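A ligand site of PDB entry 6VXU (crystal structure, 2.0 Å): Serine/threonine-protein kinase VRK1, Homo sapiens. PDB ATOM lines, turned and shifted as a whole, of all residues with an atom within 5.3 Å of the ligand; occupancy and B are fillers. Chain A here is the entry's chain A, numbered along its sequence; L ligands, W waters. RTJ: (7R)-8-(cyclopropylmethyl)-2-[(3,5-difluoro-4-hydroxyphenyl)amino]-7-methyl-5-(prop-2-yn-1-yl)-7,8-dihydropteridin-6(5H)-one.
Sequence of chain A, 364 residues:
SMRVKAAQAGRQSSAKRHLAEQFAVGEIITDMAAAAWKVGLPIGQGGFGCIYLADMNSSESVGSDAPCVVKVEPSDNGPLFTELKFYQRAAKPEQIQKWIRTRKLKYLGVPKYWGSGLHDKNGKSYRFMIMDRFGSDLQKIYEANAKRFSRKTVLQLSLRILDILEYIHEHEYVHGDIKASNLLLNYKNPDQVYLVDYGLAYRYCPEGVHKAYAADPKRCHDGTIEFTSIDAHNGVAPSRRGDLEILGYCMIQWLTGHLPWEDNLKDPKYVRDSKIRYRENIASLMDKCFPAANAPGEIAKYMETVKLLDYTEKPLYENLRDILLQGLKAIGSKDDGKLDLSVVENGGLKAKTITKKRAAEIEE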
ATOM      1  N   ILE A  43      -6.407 -17.471 -14.594  1.00  0.00           N
ATOM      2  CA  ILE A  43      -5.203 -17.403 -13.712  1.00  0.00           C
ATOM      3  C   ILE A  43      -4.416 -16.115 -14.007  1.00  0.00           C
ATOM      4  O   ILE A  43      -4.503 -15.605 -15.147  1.00  0.00           O
ATOM      5  CB  ILE A  43      -4.317 -18.654 -13.850  1.00  0.00           C
ATOM      6  CG1 ILE A  43      -3.774 -18.867 -15.271  1.00  0.00           C
ATOM      7  CG2 ILE A  43      -5.040 -19.886 -13.335  1.00  0.00           C
ATOM      8  CD1 ILE A  43      -2.524 -19.730 -15.304  1.00  0.00           C
ATOM      9  N   GLY A  44      -3.714 -15.604 -12.994  1.00  0.00           N
ATOM     10  CA  GLY A  44      -2.653 -14.585 -13.104  1.00  0.00           C
ATOM     11  C   GLY A  44      -3.098 -13.343 -13.857  1.00  0.00           C
ATOM     12  O   GLY A  44      -2.356 -12.908 -14.758  1.00  0.00           O
ATOM     13  N   PHE A  48      -1.528 -15.012 -18.890  1.00  0.00           N
ATOM     14  CA  PHE A  48      -1.126 -16.221 -19.619  1.00  0.00           C
ATOM     15  C   PHE A  48      -2.186 -16.735 -20.616  1.00  0.00           C
ATOM     16  O   PHE A  48      -2.120 -17.859 -21.080  1.00  0.00           O
ATOM     17  CB  PHE A  48      -0.761 -17.317 -18.631  1.00  0.00           C
ATOM     18  CG  PHE A  48       0.303 -16.916 -17.657  1.00  0.00           C
ATOM     19  CD1 PHE A  48      -0.039 -16.304 -16.466  1.00  0.00           C
ATOM     20  CD2 PHE A  48       1.638 -17.115 -17.950  1.00  0.00           C
ATOM     21  CE1 PHE A  48       0.947 -15.921 -15.566  1.00  0.00           C
ATOM     22  CE2 PHE A  48       2.620 -16.736 -17.059  1.00  0.00           C
ATOM     23  CZ  PHE A  48       2.273 -16.140 -15.871  1.00  0.00           C
ATOM     24  N   ILE A  51      -6.533 -19.611 -19.800  1.00  0.00           N
ATOM     25  CA  ILE A  51      -6.256 -20.659 -18.768  1.00  0.00           C
ATOM     26  C   ILE A  51      -7.047 -20.260 -17.518  1.00  0.00           C
ATOM     27  O   ILE A  51      -6.873 -19.133 -17.015  1.00  0.00           O
ATOM     28  CB  ILE A  51      -4.760 -20.787 -18.489  1.00  0.00           C
ATOM     29  CG1 ILE A  51      -3.949 -20.993 -19.777  1.00  0.00           C
ATOM     30  CG2 ILE A  51      -4.536 -21.875 -17.449  1.00  0.00           C
ATOM     31  CD1 ILE A  51      -2.459 -21.196 -19.556  1.00  0.00           C
ATOM     32  N   LEU A  53      -8.799 -21.605 -13.594  1.00  0.00           N
ATOM     33  CA  LEU A  53      -8.838 -22.576 -12.459  1.00  0.00           C
ATOM     34  C   LEU A  53      -9.953 -23.567 -12.755  1.00  0.00           C
ATOM     35  O   LEU A  53     -10.972 -23.202 -13.419  1.00  0.00           O
ATOM     36  CB  LEU A  53      -9.053 -21.840 -11.147  1.00  0.00           C
ATOM     37  CG  LEU A  53      -7.950 -20.861 -10.731  1.00  0.00           C
ATOM     38  CD1 LEU A  53      -8.418 -19.980  -9.580  1.00  0.00           C
ATOM     39  CD2 LEU A  53      -6.699 -21.618 -10.394  1.00  0.00           C
ATOM     40  N   VAL A  69      -6.064 -26.617 -13.790  1.00  0.00           N
ATOM     41  CA  VAL A  69      -6.418 -25.536 -14.740  1.00  0.00           C
ATOM     42  C   VAL A  69      -7.070 -26.188 -15.965  1.00  0.00           C
ATOM     43  O   VAL A  69      -6.817 -27.367 -16.229  1.00  0.00           O
ATOM     44  CB  VAL A  69      -5.195 -24.690 -15.136  1.00  0.00           C
ATOM     45  CG1 VAL A  69      -4.596 -24.003 -13.927  1.00  0.00           C
ATOM     46  CG2 VAL A  69      -4.138 -25.528 -15.856  1.00  0.00           C
ATOM     47  N   LYS A  71      -7.115 -25.228 -20.053  1.00  0.00           N
ATOM     48  CA  LYS A  71      -6.583 -24.396 -21.109  1.00  0.00           C
ATOM     49  C   LYS A  71      -7.607 -24.570 -22.230  1.00  0.00           C
ATOM     50  O   LYS A  71      -8.071 -25.666 -22.478  1.00  0.00           O
ATOM     51  CB  LYS A  71      -5.219 -24.905 -21.574  1.00  0.00           C
ATOM     52  CG  LYS A  71      -4.170 -24.970 -20.474  1.00  0.00           C
ATOM     53  CD  LYS A  71      -2.774 -25.204 -21.034  1.00  0.00           C
ATOM     54  CE  LYS A  71      -2.458 -24.270 -22.189  1.00  0.00           C
ATOM     55  NZ  LYS A  71      -1.009 -24.305 -22.541  1.00  0.00           N
ATOM     56  N   GLU A  83       0.360 -30.080 -28.162  1.00  0.00           N
ATOM     57  CA  GLU A  83       0.501 -30.204 -26.734  1.00  0.00           C
ATOM     58  C   GLU A  83      -0.400 -31.319 -26.188  1.00  0.00           C
ATOM     59  O   GLU A  83       0.056 -32.167 -25.429  1.00  0.00           O
ATOM     60  CB  GLU A  83       0.177 -28.873 -26.074  1.00  0.00           C
ATOM     61  CG  GLU A  83       0.404 -28.847 -24.587  1.00  0.00           C
ATOM     62  CD  GLU A  83       0.530 -27.447 -24.042  1.00  0.00           C
ATOM     63  OE1 GLU A  83      -0.461 -26.715 -24.048  1.00  0.00           O
ATOM     64  OE2 GLU A  83       1.634 -27.082 -23.597  1.00  0.00           O
ATOM     65  N   TYR A  87       0.641 -34.681 -24.161  1.00  0.00           N
ATOM     66  CA  TYR A  87       0.069 -34.937 -22.871  1.00  0.00           C
ATOM     67  C   TYR A  87      -0.699 -36.290 -22.795  1.00  0.00           C
ATOM     68  O   TYR A  87      -0.555 -37.038 -21.837  1.00  0.00           O
ATOM     69  CB  TYR A  87      -0.753 -33.705 -22.491  1.00  0.00           C
ATOM     70  CG  TYR A  87       0.063 -32.569 -21.866  1.00  0.00           C
ATOM     71  CD1 TYR A  87       1.124 -32.824 -21.033  1.00  0.00           C
ATOM     72  CD2 TYR A  87      -0.241 -31.264 -22.080  1.00  0.00           C
ATOM     73  CE1 TYR A  87       1.885 -31.826 -20.474  1.00  0.00           C
ATOM     74  CE2 TYR A  87       0.508 -30.248 -21.500  1.00  0.00           C
ATOM     75  CZ  TYR A  87       1.559 -30.539 -20.693  1.00  0.00           C
ATOM     76  OH  TYR A  87       2.287 -29.528 -20.125  1.00  0.00           O
ATOM     77  N   PRO A 111       3.890 -32.247 -16.082  1.00  0.00           N
ATOM     78  CA  PRO A 111       2.512 -32.007 -15.642  1.00  0.00           C
ATOM     79  C   PRO A 111       1.551 -33.170 -15.921  1.00  0.00           C
ATOM     80  O   PRO A 111       1.630 -33.777 -16.976  1.00  0.00           O
ATOM     81  CB  PRO A 111       2.086 -30.793 -16.451  1.00  0.00           C
ATOM     82  CG  PRO A 111       3.344 -30.098 -16.831  1.00  0.00           C
ATOM     83  CD  PRO A 111       4.434 -31.113 -16.850  1.00  0.00           C
ATOM     84  N   MET A 129      -8.372 -28.642 -22.349  1.00  0.00           N
ATOM     85  CA  MET A 129      -7.447 -29.626 -21.740  1.00  0.00           C
ATOM     86  C   MET A 129      -7.349 -29.318 -20.249  1.00  0.00           C
ATOM     87  O   MET A 129      -7.103 -28.133 -19.914  1.00  0.00           O
ATOM     88  CB  MET A 129      -6.059 -29.489 -22.394  1.00  0.00           C
ATOM     89  CG  MET A 129      -5.118 -30.601 -22.118  1.00  0.00           C
ATOM     90  SD  MET A 129      -3.623 -30.302 -23.113  1.00  0.00           S
ATOM     91  CE  MET A 129      -2.952 -28.844 -22.302  1.00  0.00           C
ATOM     92  N   MET A 131      -5.296 -29.838 -16.818  1.00  0.00           N
ATOM     93  CA  MET A 131      -3.900 -30.112 -16.375  1.00  0.00           C
ATOM     94  C   MET A 131      -3.750 -29.750 -14.898  1.00  0.00           C
ATOM     95  O   MET A 131      -4.577 -28.988 -14.385  1.00  0.00           O
ATOM     96  CB  MET A 131      -2.903 -29.259 -17.170  1.00  0.00           C
ATOM     97  CG  MET A 131      -3.015 -29.399 -18.672  1.00  0.00           C
ATOM     98  SD  MET A 131      -2.736 -31.094 -19.263  1.00  0.00           S
ATOM     99  CE  MET A 131      -1.086 -31.435 -18.660  1.00  0.00           C
ATOM    100  N   ASP A 132      -2.616 -30.107 -14.304  1.00  0.00           N
ATOM    101  CA  ASP A 132      -2.286 -29.737 -12.928  1.00  0.00           C
ATOM    102  C   ASP A 132      -2.164 -28.227 -12.743  1.00  0.00           C
ATOM    103  O   ASP A 132      -1.813 -27.503 -13.663  1.00  0.00           O
ATOM    104  CB  ASP A 132      -0.915 -30.281 -12.578  1.00  0.00           C
ATOM    105  CG  ASP A 132      -0.942 -31.707 -12.151  1.00  0.00           C
ATOM    106  OD1 ASP A 132      -2.019 -32.208 -11.792  1.00  0.00           O
ATOM    107  OD2 ASP A 132       0.120 -32.350 -12.196  1.00  0.00           O
ATOM    108  N   ARG A 133      -2.404 -27.762 -11.523  1.00  0.00           N
ATOM    109  CA  ARG A 133      -2.263 -26.343 -11.233  1.00  0.00           C
ATOM    110  C   ARG A 133      -0.973 -26.186 -10.422  1.00  0.00           C
ATOM    111  O   ARG A 133      -0.805 -26.819  -9.385  1.00  0.00           O
ATOM    112  CB  ARG A 133      -3.442 -25.815 -10.433  1.00  0.00           C
ATOM    113  CG  ARG A 133      -3.331 -24.350 -10.066  1.00  0.00           C
ATOM    114  CD  ARG A 133      -2.644 -24.187  -8.730  1.00  0.00           C
ATOM    115  NE  ARG A 133      -2.572 -22.799  -8.297  1.00  0.00           N
ATOM    116  CZ  ARG A 133      -3.545 -22.158  -7.671  1.00  0.00           C
ATOM    117  NH1 ARG A 133      -4.674 -22.783  -7.397  1.00  0.00           N
ATOM    118  NH2 ARG A 133      -3.384 -20.898  -7.318  1.00  0.00           N
ATOM    119  N   PHE A 134      -0.044 -25.364 -10.907  1.00  0.00           N
ATOM    120  CA  PHE A 134       1.218 -25.100 -10.252  1.00  0.00           C
ATOM    121  C   PHE A 134       1.277 -23.720  -9.606  1.00  0.00           C
ATOM    122  O   PHE A 134       0.329 -22.956  -9.659  1.00  0.00           O
ATOM    123  CB  PHE A 134       2.335 -25.248 -11.293  1.00  0.00           C
ATOM    124  CG  PHE A 134       2.319 -26.569 -11.963  1.00  0.00           C
ATOM    125  CD1 PHE A 134       2.758 -27.679 -11.280  1.00  0.00           C
ATOM    126  CD2 PHE A 134       1.863 -26.712 -13.251  1.00  0.00           C
ATOM    127  CE1 PHE A 134       2.744 -28.916 -11.869  1.00  0.00           C
ATOM    128  CE2 PHE A 134       1.852 -27.947 -13.854  1.00  0.00           C
ATOM    129  CZ  PHE A 134       2.293 -29.042 -13.155  1.00  0.00           C
ATOM    130  N   GLY A 135       2.378 -23.441  -8.916  1.00  0.00           N
ATOM    131  CA  GLY A 135       2.574 -22.148  -8.307  1.00  0.00           C
ATOM    132  C   GLY A 135       3.306 -21.185  -9.254  1.00  0.00           C
ATOM    133  O   GLY A 135       2.986 -21.120 -10.426  1.00  0.00           O
ATOM    134  N   SER A 136       4.292 -20.459  -8.738  1.00  0.00           N
ATOM    135  CA  SER A 136       5.068 -19.461  -9.507  1.00  0.00           C
ATOM    136  C   SER A 136       5.945 -20.147 -10.547  1.00  0.00           C
ATOM    137  O   SER A 136       6.374 -21.301 -10.318  1.00  0.00           O
ATOM    138  CB  SER A 136       5.891 -18.603  -8.578  1.00  0.00           C
ATOM    139  OG  SER A 136       6.722 -17.725  -9.318  1.00  0.00           O
ATOM    140  N   ASP A 137       6.199 -19.468 -11.699  1.00  0.00           N
ATOM    141  CA  ASP A 137       7.246 -19.857 -12.644  1.00  0.00           C
ATOM    142  C   ASP A 137       8.606 -19.400 -12.004  1.00  0.00           C
ATOM    143  O   ASP A 137       8.628 -18.486 -11.186  1.00  0.00           O
ATOM    144  CB  ASP A 137       7.028 -19.225 -14.017  1.00  0.00           C
ATOM    145  CG  ASP A 137       7.150 -17.728 -14.006  1.00  0.00           C
ATOM    146  OD1 ASP A 137       8.285 -17.237 -13.921  1.00  0.00           O
ATOM    147  OD2 ASP A 137       6.114 -17.050 -14.098  1.00  0.00           O
ATOM    148  N   SER A 181      10.933 -19.451 -17.397  1.00  0.00           N
ATOM    149  CA  SER A 181       9.509 -19.140 -17.567  1.00  0.00           C
ATOM    150  C   SER A 181       8.646 -20.380 -17.870  1.00  0.00           C
ATOM    151  O   SER A 181       7.432 -20.339 -17.717  1.00  0.00           O
ATOM    152  CB  SER A 181       9.296 -18.070 -18.628  1.00  0.00           C
ATOM    153  OG  SER A 181       9.689 -18.521 -19.904  1.00  0.00           O
ATOM    154  N   LEU A 184       7.752 -24.391 -13.482  1.00  0.00           N
ATOM    155  CA  LEU A 184       6.842 -23.987 -12.428  1.00  0.00           C
ATOM    156  C   LEU A 184       6.969 -24.854 -11.180  1.00  0.00           C
ATOM    157  O   LEU A 184       7.178 -26.055 -11.281  1.00  0.00           O
ATOM    158  CB  LEU A 184       5.387 -24.046 -12.917  1.00  0.00           C
ATOM    159  CG  LEU A 184       5.056 -23.717 -14.374  1.00  0.00           C
ATOM    160  CD1 LEU A 184       3.571 -23.835 -14.642  1.00  0.00           C
ATOM    161  CD2 LEU A 184       5.482 -22.325 -14.724  1.00  0.00           C
ATOM    162  N   VAL A 196       6.721 -27.067 -18.406  1.00  0.00           N
ATOM    163  CA  VAL A 196       5.461 -26.925 -19.129  1.00  0.00           C
ATOM    164  C   VAL A 196       5.755 -26.453 -20.565  1.00  0.00           C
ATOM    165  O   VAL A 196       6.920 -26.396 -20.943  1.00  0.00           O
ATOM    166  CB  VAL A 196       4.553 -25.913 -18.379  1.00  0.00           C
ATOM    167  CG1 VAL A 196       4.330 -26.367 -16.949  1.00  0.00           C
ATOM    168  CG2 VAL A 196       5.152 -24.526 -18.414  1.00  0.00           C
ATOM    169  N   ASP A 197       4.698 -26.204 -21.362  1.00  0.00           N
ATOM    170  CA  ASP A 197       4.745 -25.721 -22.745  1.00  0.00           C
ATOM    171  C   ASP A 197       5.299 -26.741 -23.753  1.00  0.00           C
ATOM    172  O   ASP A 197       6.468 -26.716 -24.083  1.00  0.00           O
ATOM    173  CB  ASP A 197       5.440 -24.356 -22.899  1.00  0.00           C
ATOM    174  CG  ASP A 197       5.171 -23.710 -24.230  1.00  0.00           C
ATOM    175  OD1 ASP A 197       4.741 -24.420 -25.162  1.00  0.00           O
ATOM    176  OD2 ASP A 197       5.361 -22.490 -24.352  1.00  0.00           O
HETATM  177  C4  RTJ L   1       0.352 -25.031 -18.577  1.00  0.00           C
HETATM  178  C14 RTJ L   1      -0.069 -19.879 -11.227  1.00  0.00           C
HETATM  179  C5  RTJ L   1       0.430 -26.405 -18.739  1.00  0.00           C
HETATM  180  C6  RTJ L   1       0.087 -27.212 -17.666  1.00  0.00           C
HETATM  181  C11 RTJ L   1       0.928 -19.007 -13.279  1.00  0.00           C
HETATM  182  C7  RTJ L   1      -0.546 -23.553 -14.532  1.00  0.00           C
HETATM  183  C8  RTJ L   1      -0.627 -22.281 -12.642  1.00  0.00           C
HETATM  184  C9  RTJ L   1      -0.022 -21.232 -13.304  1.00  0.00           C
HETATM  185  C10 RTJ L   1       0.305 -21.433 -14.651  1.00  0.00           C
HETATM  186  C12 RTJ L   1       1.484 -19.258 -14.664  1.00  0.00           C
HETATM  187  C13 RTJ L   1       2.997 -19.368 -14.641  1.00  0.00           C
HETATM  188  N1  RTJ L   1      -0.814 -24.761 -15.097  1.00  0.00           N
HETATM  189  N2  RTJ L   1      -0.874 -23.448 -13.236  1.00  0.00           N
HETATM  190  C3  RTJ L   1      -0.052 -24.467 -17.395  1.00  0.00           C
HETATM  191  N3  RTJ L   1       0.043 -22.600 -15.262  1.00  0.00           N
HETATM  192  C1  RTJ L   1      -0.323 -26.679 -16.467  1.00  0.00           C
HETATM  193  C2  RTJ L   1      -0.385 -25.294 -16.329  1.00  0.00           C
HETATM  194  N4  RTJ L   1       0.271 -20.024 -12.654  1.00  0.00           N
HETATM  195  N5  RTJ L   1       0.881 -20.423 -15.365  1.00  0.00           N
HETATM  196  O1  RTJ L   1       1.112 -17.920 -12.726  1.00  0.00           O
HETATM  197  F1  RTJ L   1       0.166 -28.546 -17.811  1.00  0.00           F
HETATM  198  F2  RTJ L   1       0.679 -24.231 -19.603  1.00  0.00           F
HETATM  199  O2  RTJ L   1       0.829 -26.919 -19.918  1.00  0.00           O
HETATM  200  C15 RTJ L   1      -1.499 -19.721 -10.977  1.00  0.00           C
HETATM  201  C16 RTJ L   1      -2.655 -19.615 -10.749  1.00  0.00           C
HETATM  202  C17 RTJ L   1       0.934 -20.467 -16.833  1.00  0.00           C
HETATM  203  C18 RTJ L   1       2.130 -21.193 -17.372  1.00  0.00           C
HETATM  204  C19 RTJ L   1       3.207 -20.396 -18.047  1.00  0.00           C
HETATM  205  C20 RTJ L   1       2.302 -21.260 -18.862  1.00  0.00           C
HETATM  206  O   HOH W   1      -3.487 -16.500 -10.629  1.00  0.00           O
HETATM  207  O   HOH W   2       4.329 -17.109 -12.295  1.00  0.00           O
HETATM  208  O   HOH W   3       5.551 -18.340 -17.195  1.00  0.00           O
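The backbone carbonyl oxygen of Met 131 is in hydrogen-bond range of the backbone NH of Val 69, at 2.9 Å.
OE1 of Glu 83 is in salt-bridge range of NZ of Lys 71, 2.9 Å away.
O of Ile 51 is in hydrogen-bond range of N of Ile 43 (3.0 Å).
N of Lys 71 lies within hydrogen-bond range of O of Met 129 (2.9 Å).
The backbone NH of Phe 134 is in hydrogen-bond range of a nitrogen (N2) of the ligand, at 3.1 Å.
N1 of the ligand sits at hydrogen-bond distance from O of Asp 132 (3.3 Å).
The side-chain hydroxyl of Tyr 87 sits at hydrogen-bond distance from an oxygen (O2) of the ligand, at 3.0 Å.
NZ of Lys 71 lies close to F2 of the ligand (3.4 Å).
Merely in contact with the ligand: Ile 43 (3.4 Å), Phe 48 (3.4 Å), Val 69 (3.5 Å), Glu 83 (3.8 Å), Pro 111 (3.3 Å), Met 131 (3.2 Å), Arg 133 (3.7 Å), Gly 135 (3.4 Å), Asp 137 (3.9 Å) and Leu 184 (3.8 Å).
Hydrophobic or aromatic side chains that line the ligand: Ile 43, Phe 48, Val 69, Tyr 87, Pro 111, Met 131, Phe 134 and Leu 184.
Of the 22 residues printed, 14 come within 4 Å of the ligand.
The nearest printed residue that does not touch the ligand is Val 196 (4.2 Å).
Water W3 bridges O of Ser 181 (2.8 Å) and OD2 of Asp 137 (3.4 Å).
Water W2 lies within hydrogen-bond range of OD2 of Asp 137 (2.5 Å) and O1 of the ligand (3.3 Å).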
